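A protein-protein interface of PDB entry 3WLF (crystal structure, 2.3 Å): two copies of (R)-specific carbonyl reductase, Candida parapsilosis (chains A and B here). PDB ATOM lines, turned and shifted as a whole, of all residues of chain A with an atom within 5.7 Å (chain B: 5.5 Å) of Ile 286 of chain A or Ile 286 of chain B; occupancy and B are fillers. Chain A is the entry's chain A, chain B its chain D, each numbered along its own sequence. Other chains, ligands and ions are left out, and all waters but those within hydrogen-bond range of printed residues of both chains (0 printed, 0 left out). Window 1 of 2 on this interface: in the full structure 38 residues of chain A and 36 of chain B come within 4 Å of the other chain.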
ATOM      1  N   PHE A 249      32.195  12.541 -19.453  1.00  0.00           N
ATOM      2  CA  PHE A 249      32.204  12.900 -18.042  1.00  0.00           C
ATOM      3  C   PHE A 249      33.578  13.448 -17.679  1.00  0.00           C
ATOM      4  O   PHE A 249      33.687  14.412 -16.922  1.00  0.00           O
ATOM      5  CB  PHE A 249      31.879  11.682 -17.172  1.00  0.00           C
ATOM      6  CG  PHE A 249      31.835  11.982 -15.696  1.00  0.00           C
ATOM      7  CD1 PHE A 249      33.006  12.216 -14.980  1.00  0.00           C
ATOM      8  CD2 PHE A 249      30.618  12.045 -15.024  1.00  0.00           C
ATOM      9  CE1 PHE A 249      32.968  12.508 -13.619  1.00  0.00           C
ATOM     10  CE2 PHE A 249      30.569  12.337 -13.661  1.00  0.00           C
ATOM     11  CZ  PHE A 249      31.748  12.569 -12.959  1.00  0.00           C
ATOM     12  N   VAL A 261      29.882  22.490 -10.565  1.00  0.00           N
ATOM     13  CA  VAL A 261      29.006  21.325 -10.565  1.00  0.00           C
ATOM     14  C   VAL A 261      28.944  20.591 -11.900  1.00  0.00           C
ATOM     15  O   VAL A 261      29.005  21.199 -12.969  1.00  0.00           O
ATOM     16  CB  VAL A 261      27.566  21.721 -10.161  1.00  0.00           C
ATOM     17  CG1 VAL A 261      26.967  22.647 -11.207  1.00  0.00           C
ATOM     18  CG2 VAL A 261      26.710  20.477  -9.990  1.00  0.00           C
ATOM     19  N   ILE A 262      28.826  19.271 -11.819  1.00  0.00           N
ATOM     20  CA  ILE A 262      28.726  18.419 -12.995  1.00  0.00           C
ATOM     21  C   ILE A 262      27.344  17.781 -12.934  1.00  0.00           C
ATOM     22  O   ILE A 262      26.982  17.182 -11.922  1.00  0.00           O
ATOM     23  CB  ILE A 262      29.794  17.305 -12.977  1.00  0.00           C
ATOM     24  CG1 ILE A 262      31.194  17.926 -12.966  1.00  0.00           C
ATOM     25  CG2 ILE A 262      29.623  16.399 -14.186  1.00  0.00           C
ATOM     26  CD1 ILE A 262      32.317  16.912 -12.831  1.00  0.00           C
ATOM     27  N   PRO A 264      25.311  14.982 -14.671  1.00  0.00           N
ATOM     28  CA  PRO A 264      25.217  13.851 -15.598  1.00  0.00           C
ATOM     29  C   PRO A 264      23.752  13.569 -15.916  1.00  0.00           C
ATOM     30  O   PRO A 264      23.091  12.800 -15.218  1.00  0.00           O
ATOM     31  CB  PRO A 264      25.874  12.721 -14.818  1.00  0.00           C
ATOM     32  CG  PRO A 264      25.458  13.027 -13.412  1.00  0.00           C
ATOM     33  CD  PRO A 264      25.682  14.524 -13.320  1.00  0.00           C
ATOM     34  N   PHE A 274      34.909   8.927 -11.298  1.00  0.00           N
ATOM     35  CA  PHE A 274      35.417  10.283 -11.169  1.00  0.00           C
ATOM     36  C   PHE A 274      36.741  10.259 -10.420  1.00  0.00           C
ATOM     37  O   PHE A 274      36.972   9.394  -9.574  1.00  0.00           O
ATOM     38  CB  PHE A 274      34.395  11.164 -10.437  1.00  0.00           C
ATOM     39  CG  PHE A 274      34.079  10.709  -9.033  1.00  0.00           C
ATOM     40  CD1 PHE A 274      34.935  11.008  -7.979  1.00  0.00           C
ATOM     41  CD2 PHE A 274      32.921   9.981  -8.768  1.00  0.00           C
ATOM     42  CE1 PHE A 274      34.643  10.589  -6.681  1.00  0.00           C
ATOM     43  CE2 PHE A 274      32.621   9.557  -7.475  1.00  0.00           C
ATOM     44  CZ  PHE A 274      33.484   9.862  -6.429  1.00  0.00           C
ATOM     45  N   LEU A 279      38.213  15.785  -7.500  1.00  0.00           N
ATOM     46  CA  LEU A 279      36.908  16.156  -6.970  1.00  0.00           C
ATOM     47  C   LEU A 279      36.970  16.647  -5.524  1.00  0.00           C
ATOM     48  O   LEU A 279      36.225  17.546  -5.137  1.00  0.00           O
ATOM     49  CB  LEU A 279      35.942  14.972  -7.079  1.00  0.00           C
ATOM     50  CG  LEU A 279      34.522  15.173  -6.536  1.00  0.00           C
ATOM     51  CD1 LEU A 279      33.524  14.439  -7.414  1.00  0.00           C
ATOM     52  CD2 LEU A 279      34.444  14.678  -5.101  1.00  0.00           C
ATOM     53  N   ILE A 284      34.580  19.507  -6.163  1.00  0.00           N
ATOM     54  CA  ILE A 284      33.650  19.402  -7.272  1.00  0.00           C
ATOM     55  C   ILE A 284      32.410  18.689  -6.751  1.00  0.00           C
ATOM     56  O   ILE A 284      32.492  17.895  -5.812  1.00  0.00           O
ATOM     57  CB  ILE A 284      34.258  18.583  -8.425  1.00  0.00           C
ATOM     58  CG1 ILE A 284      35.594  19.201  -8.849  1.00  0.00           C
ATOM     59  CG2 ILE A 284      33.285  18.520  -9.592  1.00  0.00           C
ATOM     60  CD1 ILE A 284      35.503  20.658  -9.262  1.00  0.00           C
ATOM     61  N   ARG A 285      31.258  18.976  -7.342  1.00  0.00           N
ATOM     62  CA  ARG A 285      30.035  18.326  -6.905  1.00  0.00           C
ATOM     63  C   ARG A 285      29.240  17.731  -8.057  1.00  0.00           C
ATOM     64  O   ARG A 285      29.027  18.376  -9.085  1.00  0.00           O
ATOM     65  CB  ARG A 285      29.177  19.305  -6.097  1.00  0.00           C
ATOM     66  CG  ARG A 285      29.072  20.706  -6.669  1.00  0.00           C
ATOM     67  CD  ARG A 285      28.815  21.711  -5.552  1.00  0.00           C
ATOM     68  NE  ARG A 285      28.657  23.073  -6.054  1.00  0.00           N
ATOM     69  CZ  ARG A 285      27.575  23.517  -6.686  1.00  0.00           C
ATOM     70  NH1 ARG A 285      26.544  22.709  -6.893  1.00  0.00           N
ATOM     71  NH2 ARG A 285      27.526  24.769  -7.117  1.00  0.00           N
ATOM     72  N   ILE A 286      28.829  16.481  -7.877  1.00  0.00           N
ATOM     73  CA  ILE A 286      28.050  15.761  -8.874  1.00  0.00           C
ATOM     74  C   ILE A 286      26.620  15.703  -8.354  1.00  0.00           C
ATOM     75  O   ILE A 286      26.367  15.149  -7.282  1.00  0.00           O
ATOM     76  CB  ILE A 286      28.563  14.311  -9.061  1.00  0.00           C
ATOM     77  CG1 ILE A 286      30.090  14.298  -9.200  1.00  0.00           C
ATOM     78  CG2 ILE A 286      27.915  13.686 -10.287  1.00  0.00           C
ATOM     79  CD1 ILE A 286      30.619  15.097 -10.366  1.00  0.00           C
ATOM     80  N   LEU A 287      25.689  16.275  -9.107  1.00  0.00           N
ATOM     81  CA  LEU A 287      24.294  16.290  -8.691  1.00  0.00           C
ATOM     82  C   LEU A 287      23.394  15.479  -9.612  1.00  0.00           C
ATOM     83  O   LEU A 287      23.409  15.656 -10.831  1.00  0.00           O
ATOM     84  CB  LEU A 287      23.781  17.733  -8.627  1.00  0.00           C
ATOM     85  CG  LEU A 287      24.598  18.724  -7.794  1.00  0.00           C
ATOM     86  CD1 LEU A 287      23.960  20.104  -7.884  1.00  0.00           C
ATOM     87  CD2 LEU A 287      24.673  18.256  -6.347  1.00  0.00           C
ATOM     88  N   GLY A 288      22.615  14.583  -9.019  1.00  0.00           N
ATOM     89  CA  GLY A 288      21.699  13.777  -9.799  1.00  0.00           C
ATOM     90  C   GLY A 288      20.458  14.603 -10.070  1.00  0.00           C
ATOM     91  O   GLY A 288      20.077  15.436  -9.249  1.00  0.00           O
ATOM     92  N   PHE B 249      32.124   3.038  -0.894  1.00  0.00           N
ATOM     93  CA  PHE B 249      31.339   4.053  -1.581  1.00  0.00           C
ATOM     94  C   PHE B 249      29.989   3.481  -2.003  1.00  0.00           C
ATOM     95  O   PHE B 249      28.975   4.176  -1.954  1.00  0.00           O
ATOM     96  CB  PHE B 249      32.093   4.589  -2.802  1.00  0.00           C
ATOM     97  CG  PHE B 249      31.339   5.644  -3.566  1.00  0.00           C
ATOM     98  CD1 PHE B 249      30.320   5.293  -4.447  1.00  0.00           C
ATOM     99  CD2 PHE B 249      31.623   6.992  -3.378  1.00  0.00           C
ATOM    100  CE1 PHE B 249      29.593   6.269  -5.126  1.00  0.00           C
ATOM    101  CE2 PHE B 249      30.903   7.977  -4.052  1.00  0.00           C
ATOM    102  CZ  PHE B 249      29.886   7.614  -4.927  1.00  0.00           C
ATOM    103  N   VAL B 261      23.296  13.243   0.530  1.00  0.00           N
ATOM    104  CA  VAL B 261      24.650  13.562   0.091  1.00  0.00           C
ATOM    105  C   VAL B 261      25.691  12.516   0.477  1.00  0.00           C
ATOM    106  O   VAL B 261      25.627  11.917   1.551  1.00  0.00           O
ATOM    107  CB  VAL B 261      25.103  14.930   0.648  1.00  0.00           C
ATOM    108  CG1 VAL B 261      25.131  14.891   2.163  1.00  0.00           C
ATOM    109  CG2 VAL B 261      26.474  15.289   0.098  1.00  0.00           C
ATOM    110  N   ILE B 262      26.648  12.306  -0.419  1.00  0.00           N
ATOM    111  CA  ILE B 262      27.734  11.360  -0.205  1.00  0.00           C
ATOM    112  C   ILE B 262      29.022  12.167  -0.184  1.00  0.00           C
ATOM    113  O   ILE B 262      29.332  12.876  -1.141  1.00  0.00           O
ATOM    114  CB  ILE B 262      27.824  10.323  -1.343  1.00  0.00           C
ATOM    115  CG1 ILE B 262      26.559   9.463  -1.372  1.00  0.00           C
ATOM    116  CG2 ILE B 262      29.055   9.446  -1.149  1.00  0.00           C
ATOM    117  CD1 ILE B 262      26.552   8.421  -2.478  1.00  0.00           C
ATOM    118  N   PRO B 264      32.903  11.689  -0.054  1.00  0.00           N
ATOM    119  CA  PRO B 264      34.070  10.804  -0.134  1.00  0.00           C
ATOM    120  C   PRO B 264      35.275  11.553   0.427  1.00  0.00           C
ATOM    121  O   PRO B 264      36.044  12.168  -0.313  1.00  0.00           O
ATOM    122  CB  PRO B 264      34.184  10.533  -1.629  1.00  0.00           C
ATOM    123  CG  PRO B 264      33.768  11.843  -2.220  1.00  0.00           C
ATOM    124  CD  PRO B 264      32.560  12.229  -1.383  1.00  0.00           C
ATOM    125  N   PHE B 274      30.118   5.485  -9.645  1.00  0.00           N
ATOM    126  CA  PHE B 274      28.803   5.567  -9.031  1.00  0.00           C
ATOM    127  C   PHE B 274      27.760   5.137 -10.051  1.00  0.00           C
ATOM    128  O   PHE B 274      27.929   5.356 -11.250  1.00  0.00           O
ATOM    129  CB  PHE B 274      28.527   7.003  -8.568  1.00  0.00           C
ATOM    130  CG  PHE B 274      28.550   8.016  -9.680  1.00  0.00           C
ATOM    131  CD1 PHE B 274      27.461   8.159 -10.536  1.00  0.00           C
ATOM    132  CD2 PHE B 274      29.671   8.812  -9.886  1.00  0.00           C
ATOM    133  CE1 PHE B 274      27.490   9.079 -11.581  1.00  0.00           C
ATOM    134  CE2 PHE B 274      29.710   9.735 -10.925  1.00  0.00           C
ATOM    135  CZ  PHE B 274      28.619   9.868 -11.775  1.00  0.00           C
ATOM    136  N   LEU B 279      21.863   7.442  -8.987  1.00  0.00           N
ATOM    137  CA  LEU B 279      22.202   8.810  -8.616  1.00  0.00           C
ATOM    138  C   LEU B 279      21.255   9.826  -9.244  1.00  0.00           C
ATOM    139  O   LEU B 279      20.890  10.816  -8.611  1.00  0.00           O
ATOM    140  CB  LEU B 279      23.647   9.119  -9.018  1.00  0.00           C
ATOM    141  CG  LEU B 279      24.130  10.565  -8.862  1.00  0.00           C
ATOM    142  CD1 LEU B 279      25.599  10.581  -8.479  1.00  0.00           C
ATOM    143  CD2 LEU B 279      23.899  11.324 -10.161  1.00  0.00           C
ATOM    144  N   ILE B 284      20.783  11.789  -5.885  1.00  0.00           N
ATOM    145  CA  ILE B 284      21.847  11.718  -4.899  1.00  0.00           C
ATOM    146  C   ILE B 284      22.925  12.705  -5.324  1.00  0.00           C
ATOM    147  O   ILE B 284      23.135  12.928  -6.516  1.00  0.00           O
ATOM    148  CB  ILE B 284      22.459  10.308  -4.846  1.00  0.00           C
ATOM    149  CG1 ILE B 284      21.384   9.299  -4.445  1.00  0.00           C
ATOM    150  CG2 ILE B 284      23.619  10.275  -3.862  1.00  0.00           C
ATOM    151  CD1 ILE B 284      21.869   7.876  -4.447  1.00  0.00           C
ATOM    152  N   ARG B 285      23.600  13.307  -4.355  1.00  0.00           N
ATOM    153  CA  ARG B 285      24.651  14.256  -4.673  1.00  0.00           C
ATOM    154  C   ARG B 285      25.964  13.926  -3.985  1.00  0.00           C
ATOM    155  O   ARG B 285      26.007  13.623  -2.794  1.00  0.00           O
ATOM    156  CB  ARG B 285      24.202  15.681  -4.333  1.00  0.00           C
ATOM    157  CG  ARG B 285      23.484  15.834  -3.010  1.00  0.00           C
ATOM    158  CD  ARG B 285      22.619  17.089  -3.028  1.00  0.00           C
ATOM    159  NE  ARG B 285      21.815  17.218  -1.818  1.00  0.00           N
ATOM    160  CZ  ARG B 285      22.305  17.521  -0.621  1.00  0.00           C
ATOM    161  NH1 ARG B 285      23.605  17.732  -0.466  1.00  0.00           N
ATOM    162  NH2 ARG B 285      21.496  17.606   0.426  1.00  0.00           N
ATOM    163  N   ILE B 286      27.035  13.964  -4.765  1.00  0.00           N
ATOM    164  CA  ILE B 286      28.369  13.683  -4.267  1.00  0.00           C
ATOM    165  C   ILE B 286      29.076  15.024  -4.166  1.00  0.00           C
ATOM    166  O   ILE B 286      29.225  15.729  -5.164  1.00  0.00           O
ATOM    167  CB  ILE B 286      29.135  12.763  -5.239  1.00  0.00           C
ATOM    168  CG1 ILE B 286      28.278  11.538  -5.572  1.00  0.00           C
ATOM    169  CG2 ILE B 286      30.455  12.329  -4.616  1.00  0.00           C
ATOM    170  CD1 ILE B 286      28.875  10.628  -6.634  1.00  0.00           C
ATOM    171  N   LEU B 287      29.499  15.384  -2.960  1.00  0.00           N
ATOM    172  CA  LEU B 287      30.167  16.660  -2.756  1.00  0.00           C
ATOM    173  C   LEU B 287      31.605  16.493  -2.276  1.00  0.00           C
ATOM    174  O   LEU B 287      31.860  15.851  -1.256  1.00  0.00           O
ATOM    175  CB  LEU B 287      29.392  17.508  -1.741  1.00  0.00           C
ATOM    176  CG  LEU B 287      27.891  17.725  -1.969  1.00  0.00           C
ATOM    177  CD1 LEU B 287      27.349  18.666  -0.901  1.00  0.00           C
ATOM    178  CD2 LEU B 287      27.648  18.304  -3.351  1.00  0.00           C
ATOM    179  N   GLY B 288      32.539  17.073  -3.021  1.00  0.00           N
ATOM    180  CA  GLY B 288      33.935  16.999  -2.636  1.00  0.00           C
ATOM    181  C   GLY B 288      34.197  18.009  -1.535  1.00  0.00           C
ATOM    182  O   GLY B 288      33.634  19.105  -1.548  1.00  0.00           O
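Of the 11 printed residues of chain A, 9 touch a printed residue of chain B.
Hydrophobic or aromatic side chains of chain A that line the printed part of chain B: Phe 249, Pro 264, Phe 274, Leu 279 and Leu 287.
Among the printed residues, no Asp or Glu carboxylate lies within 4 Å of a Lys or Arg side-chain nitrogen of the other chain.
Among the printed residues, merely in contact across the chains: Phe 249 of chain A with Phe 274 of chain B, Pro 264 of chain A with Leu 279 of chain B, Phe 274 of chain A with Phe 249 of chain B, Phe 274 of chain A with Phe 274 of chain B, Phe 274 of chain A with Ile 286 of chain B, Leu 279 of chain A with Gly 288 of chain B, Ile 284 of chain A with Ile 286 of chain B, Ile 284 of chain A with Leu 287 of chain B, Arg 285 of chain A with Ile 286 of chain B, Arg 285 of chain A with Leu 287 of chain B, Ile 286 of chain A with Ile 284 of chain B, Ile 286 of chain A with Arg 285 of chain B, Leu 287 of chain A with Arg 285 of chain B and Gly 288 of chain A with Leu 279 of chain B.
The backbone NH (N) of Gly 288 of chain B lies within hydrogen-bond range of the backbone carbonyl oxygen (O) of Ile 284 of chain A (2.9 Å).
The backbone NH of Gly 288 of chain A lies within hydrogen-bond range of the backbone carbonyl oxygen of Ile 284 of chain B, 3.0 Å away.
The backbone NH (N) of Ile 286 of chain A is in hydrogen-bond range of the backbone carbonyl oxygen (O) of Ile 286 of chain B (2.8 Å).
The backbone carbonyl oxygen (O) of Leu 279 of chain A lies within hydrogen-bond range of the backbone NH (N) of Ile 284 of chain A (2.8 Å).
The backbone carbonyl oxygen (O) of Leu 279 of chain B lies within hydrogen-bond range of the backbone NH (N) of Ile 284 of chain B (2.9 Å).
The backbone carbonyl oxygen (O) of Ile 262 of chain B sits at hydrogen-bond distance from the backbone NH (N) of Leu 287 of chain B, 3.1 Å away.
N of Ile 262 of chain A is in hydrogen-bond range of O of Arg 285 of chain A, at 2.9 Å.
The backbone carbonyl oxygen (O) of Ile 262 of chain A lies within hydrogen-bond range of the backbone NH (N) of Leu 287 of chain A, 3.2 Å away.
N of Ile 262 of chain B is in hydrogen-bond range of O of Arg 285 of chain B, at 2.8 Å.
Phe 249 of chain A touches Phe 274 of chain B, and with the chains exchanged Phe 274 of chain A touches Phe 249 of chain B.
Phe 274 of chain A touches its own counterpart, Phe 274 of chain B.
Ile 284 of chain A touches Gly 288 of chain B, and with the chains exchanged Gly 288 of chain A touches Ile 284 of chain B.
Arg 285 of chain A touches Ile 286 of chain B, and with the chains exchanged Ile 286 of chain A touches Arg 285 of chain B.
Positions printed for both chains: 249, 261, 262, 264, 274, 279, 284, 285, 286, 287 and 288.
Of the 17 pairs that touch across the chains among the printed residues, 14 have their exchanged pair printed and touching as well.
Of the printed residues of chain B, Ile 286 of chain A touches Ile 284, Arg 285 and Ile 286.
Of the printed residues of chain A, Ile 284 of chain B touches Ile 286 (3.996 Å) and Gly 288 (3.0 Å).
Printed residues of chain B within 4 Å of Pro 264 of chain A: Leu 279 (3.99 Å).
Of the printed residues of chain A, Phe 249 of chain B touches Phe 274.
Printed residues of chain A within 4 Å of Leu 287 of chain B: Ile 284 and Arg 285.
Of the printed residues of chain B, Phe 249 of chain A touches Phe 274.
The nearest printed residue of chain B that does not touch Ile 286 of chain A is Phe 274 of chain B (4.2 Å).
The nearest printed residue of chain A that does not touch Ile 286 of chain B is Leu 279 of chain A (4.7 Å).
The nearest printed residue of chain A that does not touch Ile 284 of chain B is Leu 287 of chain A (4.02 Å).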
